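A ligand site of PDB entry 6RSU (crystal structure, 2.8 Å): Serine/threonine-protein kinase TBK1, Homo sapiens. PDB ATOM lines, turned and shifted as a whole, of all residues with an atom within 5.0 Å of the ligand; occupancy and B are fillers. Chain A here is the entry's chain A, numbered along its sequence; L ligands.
SD of Met 92 lies close to N6 of the ligand (3.1 Å). OD1 of Asp 163 lies close to N5 of the ligand (3.1 Å). Asp 19 touches the ligand (CA to F1, 3.1 Å). N of Ile 20 touches F1 of the ligand (3.5 Å). Leu 21 touches the ligand. Gly 22 touches the ligand. CG2 of Val 29 touches C23 of the ligand (3.9 Å). Ala 42 touches the ligand (CB to C21, 3.4 Å). Lys 44 touches the ligand. O of Glu 93 touches C21 of the ligand (3.6 Å). Phe 94 touches the ligand (CZ to C12, 3.5 Å). Pro 96 touches the ligand (O to C4, 3.5 Å). CA of Gly 98 touches C3 of the ligand, 3.5 Å away. Hydrophobic or aromatic side chains that line the ligand: Leu 21, Val 29, Ala 42, Met 92, Phe 94 and Met 148. Within 4 Å of the ligand: Asp 19, Ile 20, Leu 21, Gly 22, Val 29, Arg 31, Ala 42, Lys 44, Met 92, Glu 93, Phe 94, Cys 95, Pro 96, Gly 98, Met 148, Thr 162 and Asp 163. The nearest printed residue that does not touch the ligand is Ser 18 (4.1 Å).
The side-chain hydroxyl (OG1) of Thr 162 sits at hydrogen-bond distance from a nitrogen (N6) of the ligand (3.0 Å). A nitrogen (N3) of the ligand sits close to the backbone carbonyl oxygen (O) of Cys 95. A nitrogen (N7) of the ligand sits close to the side-chain sulfur (SD) of Met 148 (3.7 Å). The guanidinium group of Arg 31 sits at hydrogen-bond distance from an oxygen (O1) of the ligand (3.1 Å).
N of Val 29 lies within hydrogen-bond range of O of Gly 22, at 2.9 Å. The backbone NH (N) of Leu 21 is in hydrogen-bond range of the backbone carbonyl oxygen (O) of Val 29 (3.1 Å). The backbone carbonyl oxygen (O) of Met 92 lies within hydrogen-bond range of the backbone NH (N) of Ala 42 (2.6 Å). The side-chain carboxylate (OD1) of Asp 19 is in hydrogen-bond range of the side-chain hydroxyl (OG) of Ser 18, 3.4 Å away. The backbone carbonyl oxygen of Asp 19 sits at hydrogen-bond distance from the backbone NH of Arg 31, 3.1 Å away. OD1 of Asp 163 is in salt-bridge range of NZ of Lys 44, at 3.1 Å.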
ATOM      1  N   SER A  18     -11.647  20.653  14.749  1.00  0.00           N
ATOM      2  CA  SER A  18     -11.305  20.536  13.329  1.00  0.00           C
ATOM      3  C   SER A  18      -9.804  20.479  13.086  1.00  0.00           C
ATOM      4  O   SER A  18      -9.351  19.812  12.180  1.00  0.00           O
ATOM      5  CB  SER A  18     -11.969  21.729  12.593  1.00  0.00           C
ATOM      6  OG  SER A  18     -11.257  22.125  11.435  1.00  0.00           O
ATOM      7  N   ASP A  19      -9.054  21.411  13.696  1.00  0.00           N
ATOM      8  CA  ASP A  19      -7.590  21.434  13.661  1.00  0.00           C
ATOM      9  C   ASP A  19      -7.075  20.225  14.503  1.00  0.00           C
ATOM     10  O   ASP A  19      -6.639  20.388  15.615  1.00  0.00           O
ATOM     11  CB  ASP A  19      -7.063  22.738  14.230  1.00  0.00           C
ATOM     12  CG  ASP A  19      -7.792  23.928  13.592  1.00  0.00           C
ATOM     13  OD1 ASP A  19      -8.528  23.744  12.584  1.00  0.00           O
ATOM     14  OD2 ASP A  19      -7.665  25.060  14.124  1.00  0.00           O
ATOM     15  N   ILE A  20      -6.809  19.080  13.804  1.00  0.00           N
ATOM     16  CA  ILE A  20      -6.396  17.830  14.445  1.00  0.00           C
ATOM     17  C   ILE A  20      -4.966  17.540  13.970  1.00  0.00           C
ATOM     18  O   ILE A  20      -4.651  17.765  12.816  1.00  0.00           O
ATOM     19  CB  ILE A  20      -7.260  16.655  13.918  1.00  0.00           C
ATOM     20  CG1 ILE A  20      -7.638  16.837  12.394  1.00  0.00           C
ATOM     21  CG2 ILE A  20      -8.662  16.471  14.359  1.00  0.00           C
ATOM     22  CD1 ILE A  20      -8.184  15.601  11.653  1.00  0.00           C
ATOM     23  N   LEU A  21      -4.112  17.123  14.917  1.00  0.00           N
ATOM     24  CA  LEU A  21      -2.704  16.882  14.581  1.00  0.00           C
ATOM     25  C   LEU A  21      -2.362  15.418  14.807  1.00  0.00           C
ATOM     26  O   LEU A  21      -1.532  14.866  14.041  1.00  0.00           O
ATOM     27  CB  LEU A  21      -1.777  17.752  15.476  1.00  0.00           C
ATOM     28  CG  LEU A  21      -2.100  19.250  15.479  1.00  0.00           C
ATOM     29  CD1 LEU A  21      -0.948  19.964  16.191  1.00  0.00           C
ATOM     30  CD2 LEU A  21      -2.448  19.945  14.220  1.00  0.00           C
ATOM     31  N   GLY A  22      -2.898  14.855  15.847  1.00  0.00           N
ATOM     32  CA  GLY A  22      -2.660  13.463  16.158  1.00  0.00           C
ATOM     33  C   GLY A  22      -3.784  12.767  16.893  1.00  0.00           C
ATOM     34  O   GLY A  22      -4.417  13.355  17.780  1.00  0.00           O
ATOM     35  N   VAL A  29      -4.473  14.986  20.152  1.00  0.00           N
ATOM     36  CA  VAL A  29      -3.764  16.258  20.254  1.00  0.00           C
ATOM     37  C   VAL A  29      -4.199  17.218  19.155  1.00  0.00           C
ATOM     38  O   VAL A  29      -4.117  16.822  17.970  1.00  0.00           O
ATOM     39  CB  VAL A  29      -2.247  16.015  20.244  1.00  0.00           C
ATOM     40  CG1 VAL A  29      -1.567  17.361  20.145  1.00  0.00           C
ATOM     41  CG2 VAL A  29      -1.839  15.095  21.286  1.00  0.00           C
ATOM     42  N   ARG A  31      -4.222  21.382  17.347  1.00  0.00           N
ATOM     43  CA  ARG A  31      -3.579  22.713  17.321  1.00  0.00           C
ATOM     44  C   ARG A  31      -4.432  23.700  18.183  1.00  0.00           C
ATOM     45  O   ARG A  31      -5.640  23.653  18.153  1.00  0.00           O
ATOM     46  CB  ARG A  31      -3.609  23.179  15.838  1.00  0.00           C
ATOM     47  CG  ARG A  31      -3.151  24.636  15.764  1.00  0.00           C
ATOM     48  CD  ARG A  31      -3.630  25.339  14.538  1.00  0.00           C
ATOM     49  NE  ARG A  31      -2.856  26.568  14.377  1.00  0.00           N
ATOM     50  CZ  ARG A  31      -2.144  26.852  13.269  1.00  0.00           C
ATOM     51  NH1 ARG A  31      -2.106  26.016  12.243  1.00  0.00           N
ATOM     52  NH2 ARG A  31      -1.457  27.988  13.252  1.00  0.00           N
ATOM     53  N   ALA A  42       0.571  22.287  21.496  1.00  0.00           N
ATOM     54  CA  ALA A  42      -0.108  21.038  21.130  1.00  0.00           C
ATOM     55  C   ALA A  42      -0.991  20.683  22.289  1.00  0.00           C
ATOM     56  O   ALA A  42      -0.473  20.636  23.428  1.00  0.00           O
ATOM     57  CB  ALA A  42       0.841  19.896  20.813  1.00  0.00           C
ATOM     58  N   LYS A  44      -3.045  17.981  24.342  1.00  0.00           N
ATOM     59  CA  LYS A  44      -3.343  16.557  24.512  1.00  0.00           C
ATOM     60  C   LYS A  44      -4.567  16.403  25.404  1.00  0.00           C
ATOM     61  O   LYS A  44      -4.477  16.310  26.626  1.00  0.00           O
ATOM     62  CB  LYS A  44      -2.144  15.789  25.061  1.00  0.00           C
ATOM     63  CG  LYS A  44      -2.226  14.293  24.736  1.00  0.00           C
ATOM     64  CD  LYS A  44      -0.850  13.656  24.568  1.00  0.00           C
ATOM     65  CE  LYS A  44      -0.425  12.912  25.836  1.00  0.00           C
ATOM     66  NZ  LYS A  44      -0.057  11.481  25.619  1.00  0.00           N
ATOM     67  N   VAL A  74      10.372  17.205  23.534  1.00  0.00           N
ATOM     68  CA  VAL A  74       9.219  18.081  23.568  1.00  0.00           C
ATOM     69  C   VAL A  74       8.899  18.430  25.010  1.00  0.00           C
ATOM     70  O   VAL A  74       8.779  17.558  25.880  1.00  0.00           O
ATOM     71  CB  VAL A  74       8.005  17.414  22.898  1.00  0.00           C
ATOM     72  CG1 VAL A  74       6.771  18.295  23.062  1.00  0.00           C
ATOM     73  CG2 VAL A  74       8.283  17.139  21.435  1.00  0.00           C
ATOM     74  N   MET A  92       1.490  21.031  25.406  1.00  0.00           N
ATOM     75  CA  MET A  92       2.928  20.953  25.076  1.00  0.00           C
ATOM     76  C   MET A  92       3.333  21.914  23.973  1.00  0.00           C
ATOM     77  O   MET A  92       2.492  22.399  23.206  1.00  0.00           O
ATOM     78  CB  MET A  92       3.250  19.513  24.734  1.00  0.00           C
ATOM     79  CG  MET A  92       2.305  18.521  25.424  1.00  0.00           C
ATOM     80  SD  MET A  92       2.478  16.941  24.590  1.00  0.00           S
ATOM     81  CE  MET A  92       3.910  16.337  25.482  1.00  0.00           C
ATOM     82  N   GLU A  93       4.648  22.061  23.737  1.00  0.00           N
ATOM     83  CA  GLU A  93       5.048  22.967  22.669  1.00  0.00           C
ATOM     84  C   GLU A  93       4.687  22.358  21.297  1.00  0.00           C
ATOM     85  O   GLU A  93       4.904  21.182  21.013  1.00  0.00           O
ATOM     86  CB  GLU A  93       6.550  23.217  22.769  1.00  0.00           C
ATOM     87  CG  GLU A  93       7.466  22.054  22.474  1.00  0.00           C
ATOM     88  CD  GLU A  93       8.892  22.548  22.518  1.00  0.00           C
ATOM     89  OE1 GLU A  93       9.144  23.483  21.755  1.00  0.00           O
ATOM     90  OE2 GLU A  93       9.820  21.760  22.882  1.00  0.00           O
ATOM     91  N   PHE A  94       4.108  23.235  20.455  1.00  0.00           N
ATOM     92  CA  PHE A  94       3.743  22.893  19.101  1.00  0.00           C
ATOM     93  C   PHE A  94       4.944  22.794  18.193  1.00  0.00           C
ATOM     94  O   PHE A  94       5.786  23.692  18.164  1.00  0.00           O
ATOM     95  CB  PHE A  94       2.766  23.964  18.602  1.00  0.00           C
ATOM     96  CG  PHE A  94       2.369  23.824  17.172  1.00  0.00           C
ATOM     97  CD1 PHE A  94       1.852  22.634  16.708  1.00  0.00           C
ATOM     98  CD2 PHE A  94       2.466  24.907  16.297  1.00  0.00           C
ATOM     99  CE1 PHE A  94       1.475  22.499  15.389  1.00  0.00           C
ATOM    100  CE2 PHE A  94       2.080  24.776  14.978  1.00  0.00           C
ATOM    101  CZ  PHE A  94       1.583  23.578  14.523  1.00  0.00           C
ATOM    102  N   CYS A  95       5.050  21.648  17.494  1.00  0.00           N
ATOM    103  CA  CYS A  95       6.108  21.420  16.509  1.00  0.00           C
ATOM    104  C   CYS A  95       5.566  21.684  15.111  1.00  0.00           C
ATOM    105  O   CYS A  95       4.999  20.779  14.481  1.00  0.00           O
ATOM    106  CB  CYS A  95       6.627  20.001  16.616  1.00  0.00           C
ATOM    107  SG  CYS A  95       7.193  19.520  18.273  1.00  0.00           S
ATOM    108  N   PRO A  96       5.699  22.899  14.605  1.00  0.00           N
ATOM    109  CA  PRO A  96       5.044  23.256  13.341  1.00  0.00           C
ATOM    110  C   PRO A  96       5.254  22.314  12.163  1.00  0.00           C
ATOM    111  O   PRO A  96       4.452  22.297  11.230  1.00  0.00           O
ATOM    112  CB  PRO A  96       5.676  24.620  13.017  1.00  0.00           C
ATOM    113  CG  PRO A  96       5.883  25.223  14.347  1.00  0.00           C
ATOM    114  CD  PRO A  96       6.467  24.043  15.137  1.00  0.00           C
ATOM    115  N   CYS A  97       6.332  21.544  12.190  1.00  0.00           N
ATOM    116  CA  CYS A  97       6.813  20.877  10.985  1.00  0.00           C
ATOM    117  C   CYS A  97       6.413  19.421  10.879  1.00  0.00           C
ATOM    118  O   CYS A  97       6.807  18.756   9.921  1.00  0.00           O
ATOM    119  CB  CYS A  97       8.339  21.022  10.886  1.00  0.00           C
ATOM    120  SG  CYS A  97       8.815  22.706  10.407  1.00  0.00           S
ATOM    121  N   GLY A  98       5.635  18.904  11.828  1.00  0.00           N
ATOM    122  CA  GLY A  98       5.240  17.513  11.779  1.00  0.00           C
ATOM    123  C   GLY A  98       6.172  16.547  12.480  1.00  0.00           C
ATOM    124  O   GLY A  98       6.869  16.918  13.428  1.00  0.00           O
ATOM    125  N   SER A  99       6.195  15.307  11.998  1.00  0.00           N
ATOM    126  CA  SER A  99       7.090  14.290  12.531  1.00  0.00           C
ATOM    127  C   SER A  99       8.128  13.901  11.496  1.00  0.00           C
ATOM    128  O   SER A  99       8.159  14.400  10.370  1.00  0.00           O
ATOM    129  CB  SER A  99       6.280  13.070  12.969  1.00  0.00           C
ATOM    130  OG  SER A  99       5.184  12.858  12.090  1.00  0.00           O
ATOM    131  N   THR A 102       6.311  12.347   8.636  1.00  0.00           N
ATOM    132  CA  THR A 102       5.826  13.232   7.586  1.00  0.00           C
ATOM    133  C   THR A 102       6.884  13.540   6.551  1.00  0.00           C
ATOM    134  O   THR A 102       6.602  13.609   5.351  1.00  0.00           O
ATOM    135  CB  THR A 102       5.333  14.533   8.226  1.00  0.00           C
ATOM    136  OG1 THR A 102       4.340  14.246   9.212  1.00  0.00           O
ATOM    137  CG2 THR A 102       4.807  15.470   7.161  1.00  0.00           C
ATOM    138  N   GLY A 145       6.976   8.492  13.567  1.00  0.00           N
ATOM    139  CA  GLY A 145       5.684   9.114  13.744  1.00  0.00           C
ATOM    140  C   GLY A 145       5.581   9.771  15.110  1.00  0.00           C
ATOM    141  O   GLY A 145       4.558  10.349  15.424  1.00  0.00           O
ATOM    142  N   ASN A 146       6.522   9.335  15.960  1.00  0.00           N
ATOM    143  CA  ASN A 146       6.763   9.805  17.328  1.00  0.00           C
ATOM    144  C   ASN A 146       8.061  10.574  17.537  1.00  0.00           C
ATOM    145  O   ASN A 146       8.360  10.942  18.698  1.00  0.00           O
ATOM    146  CB  ASN A 146       6.845   8.646  18.282  1.00  0.00           C
ATOM    147  CG  ASN A 146       8.178   7.947  18.148  1.00  0.00           C
ATOM    148  OD1 ASN A 146       8.295   7.289  17.241  1.00  0.00           O
ATOM    149  ND2 ASN A 146       9.178   8.108  19.006  1.00  0.00           N
ATOM    150  N   MET A 148       9.176  14.294  16.511  1.00  0.00           N
ATOM    151  CA  MET A 148       8.713  15.513  15.877  1.00  0.00           C
ATOM    152  C   MET A 148       9.869  16.404  15.444  1.00  0.00           C
ATOM    153  O   MET A 148      11.004  16.307  15.932  1.00  0.00           O
ATOM    154  CB  MET A 148       7.751  16.248  16.801  1.00  0.00           C
ATOM    155  CG  MET A 148       6.724  15.259  17.412  1.00  0.00           C
ATOM    156  SD  MET A 148       5.092  14.986  16.682  1.00  0.00           S
ATOM    157  CE  MET A 148       5.012  13.184  16.664  1.00  0.00           C
ATOM    158  N   THR A 162       8.772  12.522  22.156  1.00  0.00           N
ATOM    159  CA  THR A 162       7.543  13.141  22.657  1.00  0.00           C
ATOM    160  C   THR A 162       6.452  12.303  23.337  1.00  0.00           C
ATOM    161  O   THR A 162       5.464  12.895  23.746  1.00  0.00           O
ATOM    162  CB  THR A 162       6.746  13.876  21.526  1.00  0.00           C
ATOM    163  OG1 THR A 162       5.687  14.605  22.187  1.00  0.00           O
ATOM    164  CG2 THR A 162       6.037  12.864  20.614  1.00  0.00           C
ATOM    165  N   ASP A 163       6.424  11.027  23.283  1.00  0.00           N
ATOM    166  CA  ASP A 163       5.226  10.343  23.809  1.00  0.00           C
ATOM    167  C   ASP A 163       5.813   9.033  24.296  1.00  0.00           C
ATOM    168  O   ASP A 163       5.343   7.945  23.891  1.00  0.00           O
ATOM    169  CB  ASP A 163       4.059  10.265  22.836  1.00  0.00           C
ATOM    170  CG  ASP A 163       2.959   9.403  23.367  1.00  0.00           C
ATOM    171  OD1 ASP A 163       1.984   9.846  24.010  1.00  0.00           O
ATOM    172  OD2 ASP A 163       3.052   8.195  23.011  1.00  0.00           O
HETATM  173  C1  LIG L   1       1.737  17.521  12.029  1.00  0.00           C
HETATM  174  C2  LIG L   1      -4.489  21.790  11.562  1.00  0.00           C
HETATM  175  C3  LIG L   1       2.053  18.864  12.127  1.00  0.00           C
HETATM  176  C4  LIG L   1       2.224  19.678  10.895  1.00  0.00           C
HETATM  177  C5  LIG L   1      -2.109  22.262  11.229  1.00  0.00           C
HETATM  178  C6  LIG L   1       0.095  20.194   9.970  1.00  0.00           C
HETATM  179  C7  LIG L   1      -0.738  21.347   9.444  1.00  0.00           C
HETATM  180  C8  LIG L   1      -3.343  21.533  10.589  1.00  0.00           C
HETATM  181  N1  LIG L   1       1.975  17.399  14.299  1.00  0.00           N
HETATM  182  C9  LIG L   1       1.656  16.736  13.173  1.00  0.00           C
HETATM  183  C10 LIG L   1       2.177  18.647  14.495  1.00  0.00           C
HETATM  184  C11 LIG L   1       0.210  22.815  11.244  1.00  0.00           C
HETATM  185  C12 LIG L   1       1.010  21.602  11.749  1.00  0.00           C
HETATM  186  C13 LIG L   1       2.190  18.658   9.741  1.00  0.00           C
HETATM  187  C14 LIG L   1       2.417  19.502  13.282  1.00  0.00           C
HETATM  188  C15 LIG L   1       2.914  18.299  16.683  1.00  0.00           C
HETATM  189  C16 LIG L   1       3.195  18.181  18.692  1.00  0.00           C
HETATM  190  C17 LIG L   1       2.528  16.947  18.184  1.00  0.00           C
HETATM  191  C18 LIG L   1       2.258  15.810  18.949  1.00  0.00           C
HETATM  192  C19 LIG L   1       2.659  15.778  20.264  1.00  0.00           C
HETATM  193  C20 LIG L   1       3.296  16.866  20.814  1.00  0.00           C
HETATM  194  C21 LIG L   1       3.571  17.976  20.013  1.00  0.00           C
HETATM  195  C22 LIG L   1       2.426  14.702  21.090  1.00  0.00           C
HETATM  196  C23 LIG L   1       1.719  13.568  20.743  1.00  0.00           C
HETATM  197  C24 LIG L   1       1.527  12.575  21.698  1.00  0.00           C
HETATM  198  C25 LIG L   1       2.542  13.898  23.249  1.00  0.00           C
HETATM  199  C26 LIG L   1       1.170  12.038  19.154  1.00  0.00           C
HETATM  200  C27 LIG L   1       2.550  11.377  19.264  1.00  0.00           C
HETATM  201  C28 LIG L   1       0.821  12.471  17.750  1.00  0.00           C
HETATM  202  F1  LIG L   1      -5.611  21.195  11.234  1.00  0.00           F
HETATM  203  F2  LIG L   1      -4.720  23.095  11.585  1.00  0.00           F
HETATM  204  F3  LIG L   1      -4.221  21.537  12.821  1.00  0.00           F
HETATM  205  N2  LIG L   1      -0.974  22.117  10.597  1.00  0.00           N
HETATM  206  N3  LIG L   1       2.643  18.911  15.775  1.00  0.00           N
HETATM  207  N4  LIG L   1       3.201  18.813  17.674  1.00  0.00           N
HETATM  208  N5  LIG L   1       1.936  12.759  22.937  1.00  0.00           N
HETATM  209  N6  LIG L   1       2.741  14.854  22.365  1.00  0.00           N
HETATM  210  N7  LIG L   1       2.072  17.034  16.981  1.00  0.00           N
HETATM  211  N8  LIG L   1       1.329  20.759  10.546  1.00  0.00           N
HETATM  212  O1  LIG L   1      -2.218  22.968  12.217  1.00  0.00           O
HETATM  213  O2  LIG L   1       1.306  13.379  19.486  1.00  0.00           O
